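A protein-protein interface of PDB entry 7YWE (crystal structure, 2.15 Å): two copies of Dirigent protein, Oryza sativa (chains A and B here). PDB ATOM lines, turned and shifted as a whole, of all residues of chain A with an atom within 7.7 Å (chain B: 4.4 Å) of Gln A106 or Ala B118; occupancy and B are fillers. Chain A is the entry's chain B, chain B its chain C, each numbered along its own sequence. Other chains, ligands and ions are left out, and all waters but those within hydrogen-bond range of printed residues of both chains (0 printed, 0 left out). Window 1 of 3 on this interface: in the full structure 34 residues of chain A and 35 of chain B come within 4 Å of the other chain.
Of the 27 printed residues of chain A, 12 touch a printed residue of chain B.
Hydrophobic or aromatic side chains of chain A that line the printed part of chain B: Met A108, Val A120, Ala A127 and Met A128.
Hydrophobic or aromatic side chains of chain B within 4 Å of the printed part of chain A: His B88, Met B108, Ala B118, Val B120 and Val B132.
A ring nitrogen (ND1) of His B88 is in hydrogen-bond range of the side-chain hydroxyl of Ser A92 (2.6 Å).
A ring nitrogen (NE2) of His B88 lies within hydrogen-bond range of the backbone carbonyl oxygen (O) of Ser A90, 3.2 Å away.
The backbone carbonyl oxygen (O) of Met B108 is in hydrogen-bond range of the backbone NH (N) of Ala B118, 2.9 Å away.
O of Gly A121 is in hydrogen-bond range of N of Gln A106, at 2.9 Å.
The side-chain amide nitrogen of Gln A106 is in hydrogen-bond range of the side-chain hydroxyl of Thr A104 (3.4 Å).
The side-chain hydroxyl of Thr A104 is in hydrogen-bond range of the side-chain hydroxyl of Thr A123 (2.4 Å).
The backbone carbonyl oxygen of Gln A106 sits at hydrogen-bond distance from the backbone NH of Val A120, at 2.9 Å.
The backbone carbonyl oxygen (O) of Lys A78 sits at hydrogen-bond distance from the backbone NH (N) of Ser A92.
CG of His B88 touches O of Lys A78 (3.6 Å).
Phe A91 touches His B88 (C to CE1, 3.4 Å).
NE2 of Gln A106 touches CA of Gly B109, at 3.4 Å.
Ala B118 touches Gln A106.
Val A107 touches Met B108 (O to CE, 3.9 Å).
Met A108 touches Met B108 (SD to SD, 3.9 Å).
Gly A122 touches Val B132 (O to CG1, 3.6 Å).
CG2 of Thr A123 touches C of Trp B117, 3.5 Å away.
Thr A123 touches Ala B118.
CB of Ala A127 touches CG1 of Val B132, 3.9 Å away.
Gln A106 touches Ala B118, but with the chains exchanged Ala A118 does not touch Gln B106 (12.6 Å).
Val A107 touches Met B108, but with the chains exchanged Met A108 does not touch Val B107 (8.1 Å).
Met B108 touches its own counterpart, Met A108.
Val A120 touches its own counterpart, Val B120.
Gln A106 touches just these residues of chain B: His B88 (3.5 Å), Met B108 (3.4 Å), Gly B109 (3.4 Å) and Ala B118 (3.8 Å).
Trp A117 touches none of the printed residues of chain B.
Of the printed residues of chain B, Val A120 touches Val B120.
Ala B118 touches just these residues of chain A: Gln A106, Gly A122 and Thr A123.
Of the printed residues of chain A, Gly B131 touches Met A128.
The nearest printed residue of chain B that does not touch Gln A106 is Val B120 (4.5 Å).
The nearest residue of chain A that does not touch Ala B118 is Gly A121 (4.4 Å).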
ATOM      1  N   LYS A  78      22.598 -13.867 -15.361  1.00  0.00           N
ATOM      2  CA  LYS A  78      21.568 -14.154 -16.350  1.00  0.00           C
ATOM      3  C   LYS A  78      21.374 -12.941 -17.251  1.00  0.00           C
ATOM      4  O   LYS A  78      20.955 -11.878 -16.784  1.00  0.00           O
ATOM      5  CB  LYS A  78      20.250 -14.526 -15.672  1.00  0.00           C
ATOM      6  CG  LYS A  78      20.309 -15.788 -14.831  1.00  0.00           C
ATOM      7  CD  LYS A  78      18.968 -16.072 -14.171  1.00  0.00           C
ATOM      8  CE  LYS A  78      18.983 -17.415 -13.452  1.00  0.00           C
ATOM      9  NZ  LYS A  78      19.291 -18.527 -14.389  1.00  0.00           N
ATOM     10  N   SER A  90      25.077  -7.382 -20.668  1.00  0.00           N
ATOM     11  CA  SER A  90      23.863  -6.869 -20.048  1.00  0.00           C
ATOM     12  C   SER A  90      23.147  -8.009 -19.342  1.00  0.00           C
ATOM     13  O   SER A  90      22.503  -8.837 -19.996  1.00  0.00           O
ATOM     14  CB  SER A  90      22.948  -6.223 -21.089  1.00  0.00           C
ATOM     15  OG  SER A  90      21.676  -5.939 -20.534  1.00  0.00           O
ATOM     16  N   PHE A  91      23.256  -8.076 -18.018  1.00  0.00           N
ATOM     17  CA  PHE A  91      22.704  -9.215 -17.302  1.00  0.00           C
ATOM     18  C   PHE A  91      22.286  -8.807 -15.898  1.00  0.00           C
ATOM     19  O   PHE A  91      22.688  -7.760 -15.383  1.00  0.00           O
ATOM     20  CB  PHE A  91      23.705 -10.380 -17.252  1.00  0.00           C
ATOM     21  CG  PHE A  91      24.981 -10.067 -16.520  1.00  0.00           C
ATOM     22  CD1 PHE A  91      25.068 -10.235 -15.146  1.00  0.00           C
ATOM     23  CD2 PHE A  91      26.102  -9.636 -17.208  1.00  0.00           C
ATOM     24  CE1 PHE A  91      26.241  -9.961 -14.473  1.00  0.00           C
ATOM     25  CE2 PHE A  91      27.281  -9.360 -16.540  1.00  0.00           C
ATOM     26  CZ  PHE A  91      27.351  -9.527 -15.171  1.00  0.00           C
ATOM     27  N   SER A  92      21.464  -9.659 -15.287  1.00  0.00           N
ATOM     28  CA  SER A  92      21.046  -9.510 -13.900  1.00  0.00           C
ATOM     29  C   SER A  92      21.835 -10.493 -13.045  1.00  0.00           C
ATOM     30  O   SER A  92      21.725 -11.709 -13.233  1.00  0.00           O
ATOM     31  CB  SER A  92      19.545  -9.760 -13.746  1.00  0.00           C
ATOM     32  OG  SER A  92      18.780  -8.847 -14.514  1.00  0.00           O
ATOM     33  N   LEU A  93      22.629  -9.971 -12.112  1.00  0.00           N
ATOM     34  CA  LEU A  93      23.393 -10.812 -11.193  1.00  0.00           C
ATOM     35  C   LEU A  93      22.489 -11.154 -10.017  1.00  0.00           C
ATOM     36  O   LEU A  93      22.481 -10.474  -8.990  1.00  0.00           O
ATOM     37  CB  LEU A  93      24.667 -10.110 -10.742  1.00  0.00           C
ATOM     38  CG  LEU A  93      25.603 -10.940  -9.861  1.00  0.00           C
ATOM     39  CD1 LEU A  93      26.049 -12.195 -10.592  1.00  0.00           C
ATOM     40  CD2 LEU A  93      26.804 -10.118  -9.418  1.00  0.00           C
ATOM     41  N   VAL A  94      21.710 -12.222 -10.171  1.00  0.00           N
ATOM     42  CA  VAL A  94      20.752 -12.641  -9.153  1.00  0.00           C
ATOM     43  C   VAL A  94      21.447 -13.597  -8.191  1.00  0.00           C
ATOM     44  O   VAL A  94      21.952 -14.648  -8.600  1.00  0.00           O
ATOM     45  CB  VAL A  94      19.510 -13.286  -9.787  1.00  0.00           C
ATOM     46  CG1 VAL A  94      19.911 -14.335 -10.816  1.00  0.00           C
ATOM     47  CG2 VAL A  94      18.614 -13.889  -8.713  1.00  0.00           C
ATOM     48  N   SER A 103      17.867 -10.491  -4.052  1.00  0.00           N
ATOM     49  CA  SER A 103      18.561  -9.261  -4.401  1.00  0.00           C
ATOM     50  C   SER A 103      19.404  -9.472  -5.653  1.00  0.00           C
ATOM     51  O   SER A 103      20.158 -10.446  -5.750  1.00  0.00           O
ATOM     52  CB  SER A 103      19.437  -8.801  -3.238  1.00  0.00           C
ATOM     53  OG  SER A 103      18.676  -8.681  -2.050  1.00  0.00           O
ATOM     54  N   THR A 104      19.272  -8.562  -6.614  1.00  0.00           N
ATOM     55  CA  THR A 104      19.974  -8.660  -7.883  1.00  0.00           C
ATOM     56  C   THR A 104      20.833  -7.423  -8.108  1.00  0.00           C
ATOM     57  O   THR A 104      20.636  -6.376  -7.485  1.00  0.00           O
ATOM     58  CB  THR A 104      18.997  -8.826  -9.056  1.00  0.00           C
ATOM     59  OG1 THR A 104      18.231  -7.626  -9.219  1.00  0.00           O
ATOM     60  CG2 THR A 104      18.054  -9.994  -8.808  1.00  0.00           C
ATOM     61  N   LEU A 105      21.797  -7.564  -9.014  1.00  0.00           N
ATOM     62  CA  LEU A 105      22.651  -6.463  -9.444  1.00  0.00           C
ATOM     63  C   LEU A 105      22.600  -6.391 -10.960  1.00  0.00           C
ATOM     64  O   LEU A 105      22.900  -7.378 -11.640  1.00  0.00           O
ATOM     65  CB  LEU A 105      24.093  -6.651  -8.962  1.00  0.00           C
ATOM     66  CG  LEU A 105      24.388  -6.376  -7.486  1.00  0.00           C
ATOM     67  CD1 LEU A 105      25.800  -6.816  -7.137  1.00  0.00           C
ATOM     68  CD2 LEU A 105      24.198  -4.904  -7.175  1.00  0.00           C
ATOM     69  N   GLN A 106      22.209  -5.235 -11.487  1.00  0.00           N
ATOM     70  CA  GLN A 106      22.143  -5.031 -12.926  1.00  0.00           C
ATOM     71  C   GLN A 106      23.502  -4.558 -13.423  1.00  0.00           C
ATOM     72  O   GLN A 106      24.066  -3.596 -12.891  1.00  0.00           O
ATOM     73  CB  GLN A 106      21.048  -4.025 -13.276  1.00  0.00           C
ATOM     74  CG  GLN A 106      19.672  -4.429 -12.765  1.00  0.00           C
ATOM     75  CD  GLN A 106      19.245  -5.799 -13.262  1.00  0.00           C
ATOM     76  OE1 GLN A 106      19.477  -6.154 -14.419  1.00  0.00           O
ATOM     77  NE2 GLN A 106      18.624  -6.583 -12.385  1.00  0.00           N
ATOM     78  N   VAL A 107      24.031  -5.245 -14.430  1.00  0.00           N
ATOM     79  CA  VAL A 107      25.410  -5.062 -14.865  1.00  0.00           C
ATOM     80  C   VAL A 107      25.425  -4.769 -16.357  1.00  0.00           C
ATOM     81  O   VAL A 107      24.738  -5.439 -17.136  1.00  0.00           O
ATOM     82  CB  VAL A 107      26.269  -6.301 -14.548  1.00  0.00           C
ATOM     83  CG1 VAL A 107      27.715  -6.075 -14.969  1.00  0.00           C
ATOM     84  CG2 VAL A 107      26.183  -6.649 -13.067  1.00  0.00           C
ATOM     85  N   MET A 108      26.200  -3.763 -16.752  1.00  0.00           N
ATOM     86  CA  MET A 108      26.460  -3.479 -18.154  1.00  0.00           C
ATOM     87  C   MET A 108      27.938  -3.174 -18.317  1.00  0.00           C
ATOM     88  O   MET A 108      28.593  -2.689 -17.389  1.00  0.00           O
ATOM     89  CB  MET A 108      25.629  -2.301 -18.672  1.00  0.00           C
ATOM     90  CG  MET A 108      24.156  -2.597 -18.851  1.00  0.00           C
ATOM     91  SD  MET A 108      23.265  -1.150 -19.445  1.00  0.00           S
ATOM     92  CE  MET A 108      24.082  -0.844 -21.007  1.00  0.00           C
ATOM     93  N   TRP A 117      33.224  -3.743 -15.474  1.00  0.00           N
ATOM     94  CA  TRP A 117      31.786  -3.758 -15.681  1.00  0.00           C
ATOM     95  C   TRP A 117      31.142  -2.701 -14.796  1.00  0.00           C
ATOM     96  O   TRP A 117      31.639  -2.397 -13.709  1.00  0.00           O
ATOM     97  CB  TRP A 117      31.197  -5.134 -15.358  1.00  0.00           C
ATOM     98  CG  TRP A 117      31.198  -6.087 -16.511  1.00  0.00           C
ATOM     99  CD1 TRP A 117      31.266  -5.773 -17.836  1.00  0.00           C
ATOM    100  CD2 TRP A 117      31.120  -7.516 -16.440  1.00  0.00           C
ATOM    101  NE1 TRP A 117      31.235  -6.919 -18.596  1.00  0.00           N
ATOM    102  CE2 TRP A 117      31.149  -8.002 -17.762  1.00  0.00           C
ATOM    103  CE3 TRP A 117      31.033  -8.432 -15.387  1.00  0.00           C
ATOM    104  CZ2 TRP A 117      31.091  -9.363 -18.060  1.00  0.00           C
ATOM    105  CZ3 TRP A 117      30.977  -9.784 -15.685  1.00  0.00           C
ATOM    106  CH2 TRP A 117      31.006 -10.235 -17.010  1.00  0.00           C
ATOM    107  N   ALA A 118      30.027  -2.145 -15.264  1.00  0.00           N
ATOM    108  CA  ALA A 118      29.326  -1.088 -14.549  1.00  0.00           C
ATOM    109  C   ALA A 118      28.097  -1.648 -13.845  1.00  0.00           C
ATOM    110  O   ALA A 118      27.289  -2.355 -14.457  1.00  0.00           O
ATOM    111  CB  ALA A 118      28.911   0.038 -15.499  1.00  0.00           C
ATOM    112  N   ILE A 119      27.961  -1.323 -12.563  1.00  0.00           N
ATOM    113  CA  ILE A 119      26.757  -1.623 -11.797  1.00  0.00           C
ATOM    114  C   ILE A 119      25.768  -0.489 -12.044  1.00  0.00           C
ATOM    115  O   ILE A 119      25.935   0.617 -11.525  1.00  0.00           O
ATOM    116  CB  ILE A 119      27.066  -1.778 -10.304  1.00  0.00           C
ATOM    117  CG1 ILE A 119      28.078  -2.907 -10.085  1.00  0.00           C
ATOM    118  CG2 ILE A 119      25.789  -2.032  -9.515  1.00  0.00           C
ATOM    119  CD1 ILE A 119      28.508  -3.070  -8.644  1.00  0.00           C
ATOM    120  N   VAL A 120      24.734  -0.760 -12.846  1.00  0.00           N
ATOM    121  CA  VAL A 120      23.797   0.272 -13.274  1.00  0.00           C
ATOM    122  C   VAL A 120      22.530   0.300 -12.433  1.00  0.00           C
ATOM    123  O   VAL A 120      21.673   1.168 -12.648  1.00  0.00           O
ATOM    124  CB  VAL A 120      23.443   0.104 -14.764  1.00  0.00           C
ATOM    125  CG1 VAL A 120      24.703   0.157 -15.614  1.00  0.00           C
ATOM    126  CG2 VAL A 120      22.698  -1.203 -14.988  1.00  0.00           C
ATOM    127  N   GLY A 121      22.383  -0.615 -11.484  1.00  0.00           N
ATOM    128  CA  GLY A 121      21.193  -0.653 -10.662  1.00  0.00           C
ATOM    129  C   GLY A 121      21.118  -1.959  -9.899  1.00  0.00           C
ATOM    130  O   GLY A 121      22.046  -2.772  -9.931  1.00  0.00           O
ATOM    131  N   GLY A 122      19.997  -2.141  -9.214  1.00  0.00           N
ATOM    132  CA  GLY A 122      19.772  -3.368  -8.473  1.00  0.00           C
ATOM    133  C   GLY A 122      18.385  -3.376  -7.871  1.00  0.00           C
ATOM    134  O   GLY A 122      17.629  -2.403  -7.966  1.00  0.00           O
ATOM    135  N   THR A 123      18.057  -4.505  -7.249  1.00  0.00           N
ATOM    136  CA  THR A 123      16.768  -4.710  -6.607  1.00  0.00           C
ATOM    137  C   THR A 123      16.982  -5.344  -5.242  1.00  0.00           C
ATOM    138  O   THR A 123      18.060  -5.855  -4.929  1.00  0.00           O
ATOM    139  CB  THR A 123      15.845  -5.603  -7.447  1.00  0.00           C
ATOM    140  OG1 THR A 123      16.499  -6.851  -7.712  1.00  0.00           O
ATOM    141  CG2 THR A 123      15.487  -4.927  -8.759  1.00  0.00           C
ATOM    142  N   GLY A 124      15.934  -5.317  -4.432  1.00  0.00           N
ATOM    143  CA  GLY A 124      15.998  -5.942  -3.122  1.00  0.00           C
ATOM    144  C   GLY A 124      16.941  -5.190  -2.202  1.00  0.00           C
ATOM    145  O   GLY A 124      16.796  -3.983  -1.973  1.00  0.00           O
ATOM    146  N   PHE A 126      19.957  -4.477  -2.806  1.00  0.00           N
ATOM    147  CA  PHE A 126      20.858  -3.664  -3.615  1.00  0.00           C
ATOM    148  C   PHE A 126      20.086  -2.643  -4.445  1.00  0.00           C
ATOM    149  O   PHE A 126      20.444  -2.350  -5.587  1.00  0.00           O
ATOM    150  CB  PHE A 126      21.709  -4.545  -4.526  1.00  0.00           C
ATOM    151  CG  PHE A 126      22.631  -5.468  -3.786  1.00  0.00           C
ATOM    152  CD1 PHE A 126      23.323  -5.029  -2.671  1.00  0.00           C
ATOM    153  CD2 PHE A 126      22.800  -6.777  -4.202  1.00  0.00           C
ATOM    154  CE1 PHE A 126      24.172  -5.877  -1.987  1.00  0.00           C
ATOM    155  CE2 PHE A 126      23.646  -7.630  -3.522  1.00  0.00           C
ATOM    156  CZ  PHE A 126      24.333  -7.179  -2.413  1.00  0.00           C
ATOM    157  N   ALA A 127      19.013  -2.097  -3.881  1.00  0.00           N
ATOM    158  CA  ALA A 127      18.200  -1.132  -4.606  1.00  0.00           C
ATOM    159  C   ALA A 127      19.002   0.129  -4.901  1.00  0.00           C
ATOM    160  O   ALA A 127      19.720   0.644  -4.039  1.00  0.00           O
ATOM    161  CB  ALA A 127      16.948  -0.784  -3.804  1.00  0.00           C
ATOM    162  N   MET A 128      18.885   0.615  -6.139  1.00  0.00           N
ATOM    163  CA  MET A 128      19.525   1.858  -6.570  1.00  0.00           C
ATOM    164  C   MET A 128      21.046   1.769  -6.487  1.00  0.00           C
ATOM    165  O   MET A 128      21.734   2.787  -6.386  1.00  0.00           O
ATOM    166  CB  MET A 128      19.019   3.057  -5.761  1.00  0.00           C
ATOM    167  CG  MET A 128      17.507   3.209  -5.743  1.00  0.00           C
ATOM    168  SD  MET A 128      16.968   4.722  -4.923  1.00  0.00           S
ATOM    169  CE  MET A 128      17.610   4.469  -3.270  1.00  0.00           C
ATOM    170  N   ALA A 129      21.584   0.553  -6.542  1.00  0.00           N
ATOM    171  CA  ALA A 129      23.019   0.358  -6.393  1.00  0.00           C
ATOM    172  C   ALA A 129      23.769   0.891  -7.607  1.00  0.00           C
ATOM    173  O   ALA A 129      23.334   0.731  -8.751  1.00  0.00           O
ATOM    174  CB  ALA A 129      23.339  -1.123  -6.191  1.00  0.00           C
ATOM    175  N   THR A 130      24.903   1.531  -7.349  1.00  0.00           N
ATOM    176  CA  THR A 130      25.792   2.010  -8.394  1.00  0.00           C
ATOM    177  C   THR A 130      27.220   1.633  -8.029  1.00  0.00           C
ATOM    178  O   THR A 130      27.578   1.567  -6.850  1.00  0.00           O
ATOM    179  CB  THR A 130      25.675   3.538  -8.596  1.00  0.00           C
ATOM    180  OG1 THR A 130      26.568   3.960  -9.634  1.00  0.00           O
ATOM    181  CG2 THR A 130      26.006   4.282  -7.310  1.00  0.00           C
ATOM    182  N   GLY A 131      28.028   1.367  -9.046  1.00  0.00           N
ATOM    183  CA  GLY A 131      29.408   0.990  -8.807  1.00  0.00           C
ATOM    184  C   GLY A 131      30.002   0.331 -10.038  1.00  0.00           C
ATOM    185  O   GLY A 131      29.483   0.466 -11.144  1.00  0.00           O
ATOM    186  N   ILE A 133      32.466  -3.325 -11.409  1.00  0.00           N
ATOM    187  CA  ILE A 133      32.887  -4.700 -11.175  1.00  0.00           C
ATOM    188  C   ILE A 133      34.185  -4.921 -11.935  1.00  0.00           C
ATOM    189  O   ILE A 133      34.226  -4.763 -13.161  1.00  0.00           O
ATOM    190  CB  ILE A 133      31.821  -5.717 -11.615  1.00  0.00           C
ATOM    191  CG1 ILE A 133      30.564  -5.582 -10.750  1.00  0.00           C
ATOM    192  CG2 ILE A 133      32.375  -7.133 -11.545  1.00  0.00           C
ATOM    193  CD1 ILE A 133      29.480  -6.590 -11.078  1.00  0.00           C
ATOM    194  N   HIS B  88      15.578 -12.141 -18.392  1.00  0.00           N
ATOM    195  CA  HIS B  88      16.277 -10.889 -18.144  1.00  0.00           C
ATOM    196  C   HIS B  88      15.708  -9.814 -19.060  1.00  0.00           C
ATOM    197  O   HIS B  88      15.632 -10.005 -20.277  1.00  0.00           O
ATOM    198  CB  HIS B  88      17.780 -11.045 -18.374  1.00  0.00           C
ATOM    199  CG  HIS B  88      18.536  -9.755 -18.315  1.00  0.00           C
ATOM    200  ND1 HIS B  88      18.697  -9.038 -17.149  1.00  0.00           N
ATOM    201  CD2 HIS B  88      19.174  -9.050 -19.279  1.00  0.00           C
ATOM    202  CE1 HIS B  88      19.404  -7.949 -17.397  1.00  0.00           C
ATOM    203  NE2 HIS B  88      19.705  -7.933 -18.683  1.00  0.00           N
ATOM    204  N   GLN B 106      14.583   3.965 -17.966  1.00  0.00           N
ATOM    205  CA  GLN B 106      15.364   2.805 -18.371  1.00  0.00           C
ATOM    206  C   GLN B 106      15.273   1.726 -17.299  1.00  0.00           C
ATOM    207  O   GLN B 106      15.550   1.983 -16.123  1.00  0.00           O
ATOM    208  CB  GLN B 106      16.818   3.202 -18.624  1.00  0.00           C
ATOM    209  CG  GLN B 106      16.980   4.240 -19.718  1.00  0.00           C
ATOM    210  CD  GLN B 106      16.302   3.831 -21.014  1.00  0.00           C
ATOM    211  OE1 GLN B 106      15.541   4.602 -21.600  1.00  0.00           O
ATOM    212  NE2 GLN B 106      16.576   2.614 -21.466  1.00  0.00           N
ATOM    213  N   VAL B 107      14.876   0.522 -17.704  1.00  0.00           N
ATOM    214  CA  VAL B 107      14.542  -0.546 -16.770  1.00  0.00           C
ATOM    215  C   VAL B 107      15.316  -1.805 -17.139  1.00  0.00           C
ATOM    216  O   VAL B 107      15.340  -2.206 -18.309  1.00  0.00           O
ATOM    217  CB  VAL B 107      13.030  -0.833 -16.756  1.00  0.00           C
ATOM    218  CG1 VAL B 107      12.694  -1.868 -15.691  1.00  0.00           C
ATOM    219  CG2 VAL B 107      12.243   0.451 -16.528  1.00  0.00           C
ATOM    220  N   MET B 108      15.941  -2.424 -16.139  1.00  0.00           N
ATOM    221  CA  MET B 108      16.586  -3.721 -16.276  1.00  0.00           C
ATOM    222  C   MET B 108      16.247  -4.569 -15.061  1.00  0.00           C
ATOM    223  O   MET B 108      16.154  -4.050 -13.946  1.00  0.00           O
ATOM    224  CB  MET B 108      18.111  -3.595 -16.404  1.00  0.00           C
ATOM    225  CG  MET B 108      18.607  -3.299 -17.803  1.00  0.00           C
ATOM    226  SD  MET B 108      20.408  -3.222 -17.879  1.00  0.00           S
ATOM    227  CE  MET B 108      20.861  -4.799 -17.169  1.00  0.00           C
ATOM    228  N   GLY B 109      16.073  -5.865 -15.279  1.00  0.00           N
ATOM    229  CA  GLY B 109      15.797  -6.766 -14.179  1.00  0.00           C
ATOM    230  C   GLY B 109      15.277  -8.096 -14.676  1.00  0.00           C
ATOM    231  O   GLY B 109      15.132  -8.331 -15.879  1.00  0.00           O
ATOM    232  N   TRP B 117      11.928  -4.969 -10.565  1.00  0.00           N
ATOM    233  CA  TRP B 117      12.713  -4.401 -11.647  1.00  0.00           C
ATOM    234  C   TRP B 117      13.529  -3.235 -11.106  1.00  0.00           C
ATOM    235  O   TRP B 117      13.186  -2.634 -10.084  1.00  0.00           O
ATOM    236  CB  TRP B 117      11.823  -3.923 -12.800  1.00  0.00           C
ATOM    237  CG  TRP B 117      11.506  -4.976 -13.817  1.00  0.00           C
ATOM    238  CD1 TRP B 117      12.208  -6.121 -14.060  1.00  0.00           C
ATOM    239  CD2 TRP B 117      10.403  -4.979 -14.731  1.00  0.00           C
ATOM    240  NE1 TRP B 117      11.611  -6.835 -15.071  1.00  0.00           N
ATOM    241  CE2 TRP B 117      10.501  -6.154 -15.500  1.00  0.00           C
ATOM    242  CE3 TRP B 117       9.344  -4.098 -14.975  1.00  0.00           C
ATOM    243  CZ2 TRP B 117       9.579  -6.473 -16.493  1.00  0.00           C
ATOM    244  CZ3 TRP B 117       8.430  -4.417 -15.961  1.00  0.00           C
ATOM    245  CH2 TRP B 117       8.553  -5.594 -16.709  1.00  0.00           C
ATOM    246  N   ALA B 118      14.617  -2.920 -11.796  1.00  0.00           N
ATOM    247  CA  ALA B 118      15.508  -1.841 -11.393  1.00  0.00           C
ATOM    248  C   ALA B 118      15.444  -0.707 -12.405  1.00  0.00           C
ATOM    249  O   ALA B 118      15.433  -0.941 -13.618  1.00  0.00           O
ATOM    250  CB  ALA B 118      16.950  -2.335 -11.252  1.00  0.00           C
ATOM    251  N   ILE B 119      15.387   0.518 -11.894  1.00  0.00           N
ATOM    252  CA  ILE B 119      15.424   1.720 -12.717  1.00  0.00           C
ATOM    253  C   ILE B 119      16.883   2.150 -12.817  1.00  0.00           C
ATOM    254  O   ILE B 119      17.508   2.497 -11.814  1.00  0.00           O
ATOM    255  CB  ILE B 119      14.550   2.832 -12.127  1.00  0.00           C
ATOM    256  CG1 ILE B 119      13.087   2.387 -12.093  1.00  0.00           C
ATOM    257  CG2 ILE B 119      14.707   4.128 -12.915  1.00  0.00           C
ATOM    258  CD1 ILE B 119      12.172   3.398 -11.461  1.00  0.00           C
ATOM    259  N   VAL B 120      17.432   2.113 -14.032  1.00  0.00           N
ATOM    260  CA  VAL B 120      18.851   2.366 -14.236  1.00  0.00           C
ATOM    261  C   VAL B 120      19.115   3.728 -14.856  1.00  0.00           C
ATOM    262  O   VAL B 120      20.282   4.100 -15.041  1.00  0.00           O
ATOM    263  CB  VAL B 120      19.482   1.248 -15.090  1.00  0.00           C
ATOM    264  CG1 VAL B 120      19.241  -0.104 -14.437  1.00  0.00           C
ATOM    265  CG2 VAL B 120      18.901   1.263 -16.486  1.00  0.00           C
ATOM    266  N   GLY B 131      15.928   3.896  -9.105  1.00  0.00           N
ATOM    267  CA  GLY B 131      14.932   3.313  -8.227  1.00  0.00           C
ATOM    268  C   GLY B 131      14.606   1.894  -8.643  1.00  0.00           C
ATOM    269  O   GLY B 131      15.399   1.229  -9.311  1.00  0.00           O
ATOM    270  N   VAL B 132      13.420   1.442  -8.229  1.00  0.00           N
ATOM    271  CA  VAL B 132      12.966   0.082  -8.480  1.00  0.00           C
ATOM    272  C   VAL B 132      11.517   0.112  -8.944  1.00  0.00           C
ATOM    273  O   VAL B 132      10.768   1.054  -8.672  1.00  0.00           O
ATOM    274  CB  VAL B 132      13.107  -0.821  -7.235  1.00  0.00           C
ATOM    275  CG1 VAL B 132      14.570  -0.969  -6.842  1.00  0.00           C
ATOM    276  CG2 VAL B 132      12.293  -0.264  -6.079  1.00  0.00           C
